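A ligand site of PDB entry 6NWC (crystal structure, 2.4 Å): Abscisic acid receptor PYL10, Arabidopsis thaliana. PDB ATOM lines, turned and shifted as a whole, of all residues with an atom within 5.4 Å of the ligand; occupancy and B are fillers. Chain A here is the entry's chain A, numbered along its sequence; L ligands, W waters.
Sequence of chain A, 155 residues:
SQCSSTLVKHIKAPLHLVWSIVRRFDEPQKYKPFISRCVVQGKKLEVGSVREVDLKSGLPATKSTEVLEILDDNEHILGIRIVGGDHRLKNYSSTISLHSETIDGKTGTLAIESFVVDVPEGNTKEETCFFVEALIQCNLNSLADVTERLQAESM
A ring nitrogen (ND1) of His 87 is in hydrogen-bond range of the backbone NH of Leu 89, 3.2 Å away. The backbone carbonyl oxygen (O) of Tyr 92 is in hydrogen-bond range of the backbone NH (N) of Ile 82, 3.0 Å away. The side-chain hydroxyl of Ser 64 sits at hydrogen-bond distance from the side-chain carboxylate of Glu 66, at 2.8 Å. The side-chain amide nitrogen (ND2) of Asn 139 lies close to the backbone carbonyl oxygen (O) of Leu 135, at 3.5 Å.
ND2 of Asn 139 is in hydrogen-bond range of O1 of the ligand, at 2.8 Å. The side-chain amino group (NZ) of Lys 32 is in salt-bridge range of an oxygen (O2) of the ligand.
Water W1 lies within hydrogen-bond range of the side-chain amide oxygen of Asn 139 (2.6 Å), an oxygen (O1) of the ligand (2.9 Å) and the backbone NH of Phe 34 (3.0 Å). Water W2 bridges the side-chain carboxylate of Glu 66 (2.8 Å) and a nitrogen (N2) of the ligand (3.1 Å).
Merely in contact with the ligand: Leu 55, Leu 59, Ser 64, Ile 82, His 87, Leu 89, Tyr 92, Glu 113, Val 132, Leu 135 and Ile 136. Hydrophobic or aromatic side chains within 4 Å of the ligand: Leu 55, Leu 59, Ile 82, His 87, Leu 89, Tyr 92, Val 132, Leu 135 and Ile 136. Within 4 Å of the ligand: Lys 32, Leu 55, Leu 59, Ser 64, Ile 82, His 87, Leu 89, Tyr 92, Glu 113, Val 132, Leu 135, Ile 136 and Asn 139. The nearest printed residue that does not touch the ligand is Ile 35 (4.03 Å).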
ATOM      1  N   LYS A  32      14.867 -12.075  -3.342  1.00  0.00           N
ATOM      2  CA  LYS A  32      14.477 -12.822  -2.161  1.00  0.00           C
ATOM      3  C   LYS A  32      12.995 -13.163  -2.273  1.00  0.00           C
ATOM      4  O   LYS A  32      12.157 -12.251  -2.198  1.00  0.00           O
ATOM      5  CB  LYS A  32      14.755 -12.022  -0.901  1.00  0.00           C
ATOM      6  CG  LYS A  32      16.237 -11.880  -0.593  1.00  0.00           C
ATOM      7  CD  LYS A  32      16.448 -11.240   0.763  1.00  0.00           C
ATOM      8  CE  LYS A  32      17.923 -11.194   1.161  1.00  0.00           C
ATOM      9  NZ  LYS A  32      18.072 -10.667   2.561  1.00  0.00           N
ATOM     10  N   PHE A  34      10.534 -14.297  -0.569  1.00  0.00           N
ATOM     11  CA  PHE A  34       9.536 -14.160   0.483  1.00  0.00           C
ATOM     12  C   PHE A  34       9.322 -12.724   0.906  1.00  0.00           C
ATOM     13  O   PHE A  34       8.626 -12.486   1.897  1.00  0.00           O
ATOM     14  CB  PHE A  34       9.946 -14.988   1.696  1.00  0.00           C
ATOM     15  CG  PHE A  34      10.174 -16.441   1.391  1.00  0.00           C
ATOM     16  CD1 PHE A  34       9.161 -17.219   0.854  1.00  0.00           C
ATOM     17  CD2 PHE A  34      11.406 -17.025   1.647  1.00  0.00           C
ATOM     18  CE1 PHE A  34       9.365 -18.553   0.576  1.00  0.00           C
ATOM     19  CE2 PHE A  34      11.616 -18.357   1.378  1.00  0.00           C
ATOM     20  CZ  PHE A  34      10.587 -19.128   0.837  1.00  0.00           C
ATOM     21  N   ILE A  35       9.919 -11.770   0.202  1.00  0.00           N
ATOM     22  CA  ILE A  35       9.792 -10.363   0.533  1.00  0.00           C
ATOM     23  C   ILE A  35       9.008  -9.701  -0.577  1.00  0.00           C
ATOM     24  O   ILE A  35       9.348  -9.827  -1.756  1.00  0.00           O
ATOM     25  CB  ILE A  35      11.167  -9.691   0.705  1.00  0.00           C
ATOM     26  CG1 ILE A  35      11.818 -10.183   1.993  1.00  0.00           C
ATOM     27  CG2 ILE A  35      11.017  -8.178   0.654  1.00  0.00           C
ATOM     28  CD1 ILE A  35      13.265  -9.806   2.134  1.00  0.00           C
ATOM     29  N   ARG A  51      15.838  -0.336   6.752  1.00  0.00           N
ATOM     30  CA  ARG A  51      14.797  -0.721   5.819  1.00  0.00           C
ATOM     31  C   ARG A  51      13.656  -1.358   6.581  1.00  0.00           C
ATOM     32  O   ARG A  51      13.860  -2.086   7.553  1.00  0.00           O
ATOM     33  CB  ARG A  51      15.320  -1.681   4.745  1.00  0.00           C
ATOM     34  CG  ARG A  51      15.808  -3.023   5.240  1.00  0.00           C
ATOM     35  CD  ARG A  51      16.440  -3.792   4.083  1.00  0.00           C
ATOM     36  NE  ARG A  51      16.960  -5.084   4.481  1.00  0.00           N
ATOM     37  CZ  ARG A  51      17.604  -5.914   3.665  1.00  0.00           C
ATOM     38  NH1 ARG A  51      18.058  -7.082   4.118  1.00  0.00           N
ATOM     39  NH2 ARG A  51      17.793  -5.577   2.397  1.00  0.00           N
ATOM     40  N   LEU A  55       6.773  -8.661   4.238  1.00  0.00           N
ATOM     41  CA  LEU A  55       6.901 -10.020   3.733  1.00  0.00           C
ATOM     42  C   LEU A  55       5.672 -10.405   2.919  1.00  0.00           C
ATOM     43  O   LEU A  55       4.639  -9.724   2.936  1.00  0.00           O
ATOM     44  CB  LEU A  55       7.092 -11.002   4.887  1.00  0.00           C
ATOM     45  CG  LEU A  55       8.274 -10.720   5.820  1.00  0.00           C
ATOM     46  CD1 LEU A  55       8.226 -11.636   7.038  1.00  0.00           C
ATOM     47  CD2 LEU A  55       9.577 -10.880   5.057  1.00  0.00           C
ATOM     48  N   LEU A  59       2.673 -16.113   5.587  1.00  0.00           N
ATOM     49  CA  LEU A  59       3.885 -16.470   6.289  1.00  0.00           C
ATOM     50  C   LEU A  59       3.697 -16.234   7.783  1.00  0.00           C
ATOM     51  O   LEU A  59       2.793 -15.493   8.192  1.00  0.00           O
ATOM     52  CB  LEU A  59       5.080 -15.646   5.793  1.00  0.00           C
ATOM     53  CG  LEU A  59       6.051 -16.335   4.840  1.00  0.00           C
ATOM     54  CD1 LEU A  59       5.478 -16.421   3.433  1.00  0.00           C
ATOM     55  CD2 LEU A  59       7.400 -15.621   4.834  1.00  0.00           C
ATOM     56  N   PRO A  60       4.517 -16.869   8.625  1.00  0.00           N
ATOM     57  CA  PRO A  60       4.415 -16.628  10.083  1.00  0.00           C
ATOM     58  C   PRO A  60       4.529 -15.173  10.495  1.00  0.00           C
ATOM     59  O   PRO A  60       4.100 -14.846  11.614  1.00  0.00           O
ATOM     60  CB  PRO A  60       5.582 -17.458  10.641  1.00  0.00           C
ATOM     61  CG  PRO A  60       5.719 -18.596   9.668  1.00  0.00           C
ATOM     62  CD  PRO A  60       5.346 -18.050   8.309  1.00  0.00           C
ATOM     63  N   ALA A  61       5.102 -14.295   9.676  1.00  0.00           N
ATOM     64  CA  ALA A  61       5.267 -12.904  10.042  1.00  0.00           C
ATOM     65  C   ALA A  61       5.031 -12.029   8.821  1.00  0.00           C
ATOM     66  O   ALA A  61       4.979 -12.524   7.694  1.00  0.00           O
ATOM     67  CB  ALA A  61       6.653 -12.637  10.637  1.00  0.00           C
ATOM     68  N   LYS A  63       6.182  -8.193   8.869  1.00  0.00           N
ATOM     69  CA  LYS A  63       7.061  -7.040   8.828  1.00  0.00           C
ATOM     70  C   LYS A  63       8.434  -7.407   9.357  1.00  0.00           C
ATOM     71  O   LYS A  63       8.579  -8.292  10.197  1.00  0.00           O
ATOM     72  CB  LYS A  63       6.491  -5.874   9.663  1.00  0.00           C
ATOM     73  CG  LYS A  63       5.321  -5.155   9.009  1.00  0.00           C
ATOM     74  CD  LYS A  63       4.758  -4.018   9.845  1.00  0.00           C
ATOM     75  CE  LYS A  63       3.732  -3.197   9.053  1.00  0.00           C
ATOM     76  NZ  LYS A  63       4.304  -2.559   7.807  1.00  0.00           N
ATOM     77  N   SER A  64       9.449  -6.693   8.864  1.00  0.00           N
ATOM     78  CA  SER A  64      10.798  -6.776   9.418  1.00  0.00           C
ATOM     79  C   SER A  64      11.462  -5.412   9.267  1.00  0.00           C
ATOM     80  O   SER A  64      11.303  -4.750   8.241  1.00  0.00           O
ATOM     81  CB  SER A  64      11.617  -7.886   8.732  1.00  0.00           C
ATOM     82  OG  SER A  64      12.916  -8.041   9.288  1.00  0.00           O
ATOM     83  N   GLU A  66      15.290  -3.718   9.520  1.00  0.00           N
ATOM     84  CA  GLU A  66      16.668  -4.173   9.458  1.00  0.00           C
ATOM     85  C   GLU A  66      17.622  -2.999   9.235  1.00  0.00           C
ATOM     86  O   GLU A  66      17.277  -2.008   8.586  1.00  0.00           O
ATOM     87  CB  GLU A  66      16.829  -5.225   8.348  1.00  0.00           C
ATOM     88  CG  GLU A  66      15.523  -5.981   8.098  1.00  0.00           C
ATOM     89  CD  GLU A  66      15.631  -7.156   7.129  1.00  0.00           C
ATOM     90  OE1 GLU A  66      16.413  -7.086   6.167  1.00  0.00           O
ATOM     91  OE2 GLU A  66      14.899  -8.149   7.352  1.00  0.00           O
ATOM     92  N   ILE A  82      18.761  -7.539  11.938  1.00  0.00           N
ATOM     93  CA  ILE A  82      17.319  -7.377  12.090  1.00  0.00           C
ATOM     94  C   ILE A  82      17.021  -6.904  13.518  1.00  0.00           C
ATOM     95  O   ILE A  82      17.545  -7.481  14.480  1.00  0.00           O
ATOM     96  CB  ILE A  82      16.592  -8.690  11.776  1.00  0.00           C
ATOM     97  CG1 ILE A  82      16.714  -8.992  10.281  1.00  0.00           C
ATOM     98  CG2 ILE A  82      15.168  -8.605  12.206  1.00  0.00           C
ATOM     99  CD1 ILE A  82      16.360 -10.454   9.915  1.00  0.00           C
ATOM    100  N   HIS A  87       8.059 -11.076  13.912  1.00  0.00           N
ATOM    101  CA  HIS A  87       8.647 -12.399  13.748  1.00  0.00           C
ATOM    102  C   HIS A  87       9.294 -12.828  15.061  1.00  0.00           C
ATOM    103  O   HIS A  87       9.370 -12.066  16.023  1.00  0.00           O
ATOM    104  CB  HIS A  87       9.679 -12.381  12.622  1.00  0.00           C
ATOM    105  CG  HIS A  87      10.709 -11.300  12.804  1.00  0.00           C
ATOM    106  ND1 HIS A  87      11.827 -11.465  13.589  1.00  0.00           N
ATOM    107  CD2 HIS A  87      10.753 -10.025  12.337  1.00  0.00           C
ATOM    108  CE1 HIS A  87      12.522 -10.348  13.598  1.00  0.00           C
ATOM    109  NE2 HIS A  87      11.901  -9.457  12.842  1.00  0.00           N
ATOM    110  N   LEU A  89      12.509 -13.859  15.637  1.00  0.00           N
ATOM    111  CA  LEU A  89      13.969 -13.890  15.640  1.00  0.00           C
ATOM    112  C   LEU A  89      14.526 -12.727  16.457  1.00  0.00           C
ATOM    113  O   LEU A  89      14.165 -11.572  16.228  1.00  0.00           O
ATOM    114  CB  LEU A  89      14.521 -13.846  14.224  1.00  0.00           C
ATOM    115  CG  LEU A  89      14.112 -15.031  13.384  1.00  0.00           C
ATOM    116  CD1 LEU A  89      14.554 -14.835  11.971  1.00  0.00           C
ATOM    117  CD2 LEU A  89      14.763 -16.248  13.958  1.00  0.00           C
ATOM    118  N   TYR A  92      19.321 -11.462  15.313  1.00  0.00           N
ATOM    119  CA  TYR A  92      19.773 -11.963  14.020  1.00  0.00           C
ATOM    120  C   TYR A  92      20.686 -10.924  13.373  1.00  0.00           C
ATOM    121  O   TYR A  92      20.273  -9.788  13.172  1.00  0.00           O
ATOM    122  CB  TYR A  92      18.566 -12.267  13.133  1.00  0.00           C
ATOM    123  CG  TYR A  92      18.908 -12.839  11.760  1.00  0.00           C
ATOM    124  CD1 TYR A  92      19.216 -12.008  10.690  1.00  0.00           C
ATOM    125  CD2 TYR A  92      18.891 -14.216  11.547  1.00  0.00           C
ATOM    126  CE1 TYR A  92      19.513 -12.530   9.436  1.00  0.00           C
ATOM    127  CE2 TYR A  92      19.195 -14.745  10.302  1.00  0.00           C
ATOM    128  CZ  TYR A  92      19.497 -13.894   9.244  1.00  0.00           C
ATOM    129  OH  TYR A  92      19.799 -14.413   7.998  1.00  0.00           O
ATOM    130  N   GLU A 113      26.967 -16.781   2.848  1.00  0.00           N
ATOM    131  CA  GLU A 113      26.178 -16.021   3.808  1.00  0.00           C
ATOM    132  C   GLU A 113      26.230 -16.730   5.155  1.00  0.00           C
ATOM    133  O   GLU A 113      25.719 -17.848   5.278  1.00  0.00           O
ATOM    134  CB  GLU A 113      24.728 -15.872   3.334  1.00  0.00           C
ATOM    135  CG  GLU A 113      23.835 -15.154   4.313  1.00  0.00           C
ATOM    136  CD  GLU A 113      22.549 -14.622   3.684  1.00  0.00           C
ATOM    137  OE1 GLU A 113      22.490 -14.563   2.444  1.00  0.00           O
ATOM    138  OE2 GLU A 113      21.606 -14.262   4.434  1.00  0.00           O
ATOM    139  N   PHE A 131      15.621 -23.994  10.386  1.00  0.00           N
ATOM    140  CA  PHE A 131      14.611 -23.225   9.671  1.00  0.00           C
ATOM    141  C   PHE A 131      15.228 -22.044   8.924  1.00  0.00           C
ATOM    142  O   PHE A 131      14.803 -21.725   7.805  1.00  0.00           O
ATOM    143  CB  PHE A 131      13.557 -22.746  10.670  1.00  0.00           C
ATOM    144  CG  PHE A 131      12.370 -22.070  10.037  1.00  0.00           C
ATOM    145  CD1 PHE A 131      11.949 -22.452   8.756  1.00  0.00           C
ATOM    146  CD2 PHE A 131      11.695 -21.054  10.695  1.00  0.00           C
ATOM    147  CE1 PHE A 131      10.859 -21.843   8.171  1.00  0.00           C
ATOM    148  CE2 PHE A 131      10.603 -20.436  10.109  1.00  0.00           C
ATOM    149  CZ  PHE A 131      10.192 -20.814   8.844  1.00  0.00           C
ATOM    150  N   VAL A 132      16.254 -21.414   9.500  1.00  0.00           N
ATOM    151  CA  VAL A 132      16.865 -20.246   8.860  1.00  0.00           C
ATOM    152  C   VAL A 132      17.742 -20.665   7.685  1.00  0.00           C
ATOM    153  O   VAL A 132      17.753 -20.021   6.631  1.00  0.00           O
ATOM    154  CB  VAL A 132      17.674 -19.431   9.893  1.00  0.00           C
ATOM    155  CG1 VAL A 132      18.464 -18.340   9.208  1.00  0.00           C
ATOM    156  CG2 VAL A 132      16.742 -18.849  10.944  1.00  0.00           C
ATOM    157  N   LEU A 135      15.658 -21.219   4.588  1.00  0.00           N
ATOM    158  CA  LEU A 135      15.234 -19.954   3.992  1.00  0.00           C
ATOM    159  C   LEU A 135      16.383 -19.272   3.250  1.00  0.00           C
ATOM    160  O   LEU A 135      16.173 -18.698   2.169  1.00  0.00           O
ATOM    161  CB  LEU A 135      14.685 -19.028   5.092  1.00  0.00           C
ATOM    162  CG  LEU A 135      13.500 -19.581   5.865  1.00  0.00           C
ATOM    163  CD1 LEU A 135      12.811 -18.492   6.689  1.00  0.00           C
ATOM    164  CD2 LEU A 135      12.528 -20.241   4.898  1.00  0.00           C
ATOM    165  N   ILE A 136      17.592 -19.323   3.808  1.00  0.00           N
ATOM    166  CA  ILE A 136      18.723 -18.668   3.173  1.00  0.00           C
ATOM    167  C   ILE A 136      19.093 -19.391   1.890  1.00  0.00           C
ATOM    168  O   ILE A 136      19.341 -18.766   0.848  1.00  0.00           O
ATOM    169  CB  ILE A 136      19.900 -18.588   4.157  1.00  0.00           C
ATOM    170  CG1 ILE A 136      19.589 -17.579   5.258  1.00  0.00           C
ATOM    171  CG2 ILE A 136      21.180 -18.204   3.444  1.00  0.00           C
ATOM    172  CD1 ILE A 136      20.705 -17.390   6.234  1.00  0.00           C
ATOM    173  N   ASN A 139      16.919 -18.307  -0.658  1.00  0.00           N
ATOM    174  CA  ASN A 139      17.318 -16.976  -1.126  1.00  0.00           C
ATOM    175  C   ASN A 139      18.517 -17.070  -2.068  1.00  0.00           C
ATOM    176  O   ASN A 139      18.581 -16.325  -3.045  1.00  0.00           O
ATOM    177  CB  ASN A 139      17.631 -16.051   0.055  1.00  0.00           C
ATOM    178  CG  ASN A 139      16.375 -15.578   0.762  1.00  0.00           C
ATOM    179  OD1 ASN A 139      15.295 -15.553   0.169  1.00  0.00           O
ATOM    180  ND2 ASN A 139      16.503 -15.220   2.030  1.00  0.00           N
HETATM  181  C1  LIG L   1      11.100 -13.666   7.975  1.00  0.00           C
HETATM  182  C2  LIG L   1      10.478 -14.899   7.854  1.00  0.00           C
HETATM  183  C3  LIG L   1      10.519 -15.585   6.644  1.00  0.00           C
HETATM  184  C4  LIG L   1      11.175 -15.030   5.544  1.00  0.00           C
HETATM  185  C5  LIG L   1      11.813 -13.795   5.653  1.00  0.00           C
HETATM  186  C6  LIG L   1      11.756 -13.111   6.876  1.00  0.00           C
HETATM  187  C7  LIG L   1       9.792 -15.447   8.998  1.00  0.00           C
HETATM  188  C8  LIG L   1      11.029 -12.985   9.195  1.00  0.00           C
HETATM  189  C9  LIG L   1      11.798 -11.662   9.279  1.00  0.00           C
HETATM  190  C10 LIG L   1      12.308 -12.896  10.031  1.00  0.00           C
HETATM  191  C11 LIG L   1      12.474 -13.229   4.547  1.00  0.00           C
HETATM  192  C12 LIG L   1      13.979 -13.583   4.509  1.00  0.00           C
HETATM  193  C13 LIG L   1      16.137 -13.573   5.791  1.00  0.00           C
HETATM  194  C14 LIG L   1      16.295 -15.296   8.136  1.00  0.00           C
HETATM  195  C15 LIG L   1      15.871 -15.829   6.768  1.00  0.00           C
HETATM  196  C16 LIG L   1      16.534 -15.048   5.660  1.00  0.00           C
HETATM  197  C17 LIG L   1      16.591 -13.043   7.165  1.00  0.00           C
HETATM  198  C18 LIG L   1      15.895 -13.833   8.260  1.00  0.00           C
HETATM  199  C19 LIG L   1      16.846 -12.727   4.724  1.00  0.00           C
HETATM  200  N1  LIG L   1       9.258 -15.876   9.933  1.00  0.00           N
HETATM  201  N2  LIG L   1      14.674 -13.368   5.650  1.00  0.00           N
HETATM  202  O1  LIG L   1      14.486 -14.020   3.473  1.00  0.00           O
HETATM  203  O2  LIG L   1      16.310 -11.626   4.418  1.00  0.00           O
HETATM  204  O3  LIG L   1      17.896 -13.177   4.218  1.00  0.00           O
HETATM  205  O   HOH W   1      13.099 -14.368   0.908  1.00  0.00           O
HETATM  206  O   HOH W   2      13.820 -10.456   6.249  1.00  0.00           O
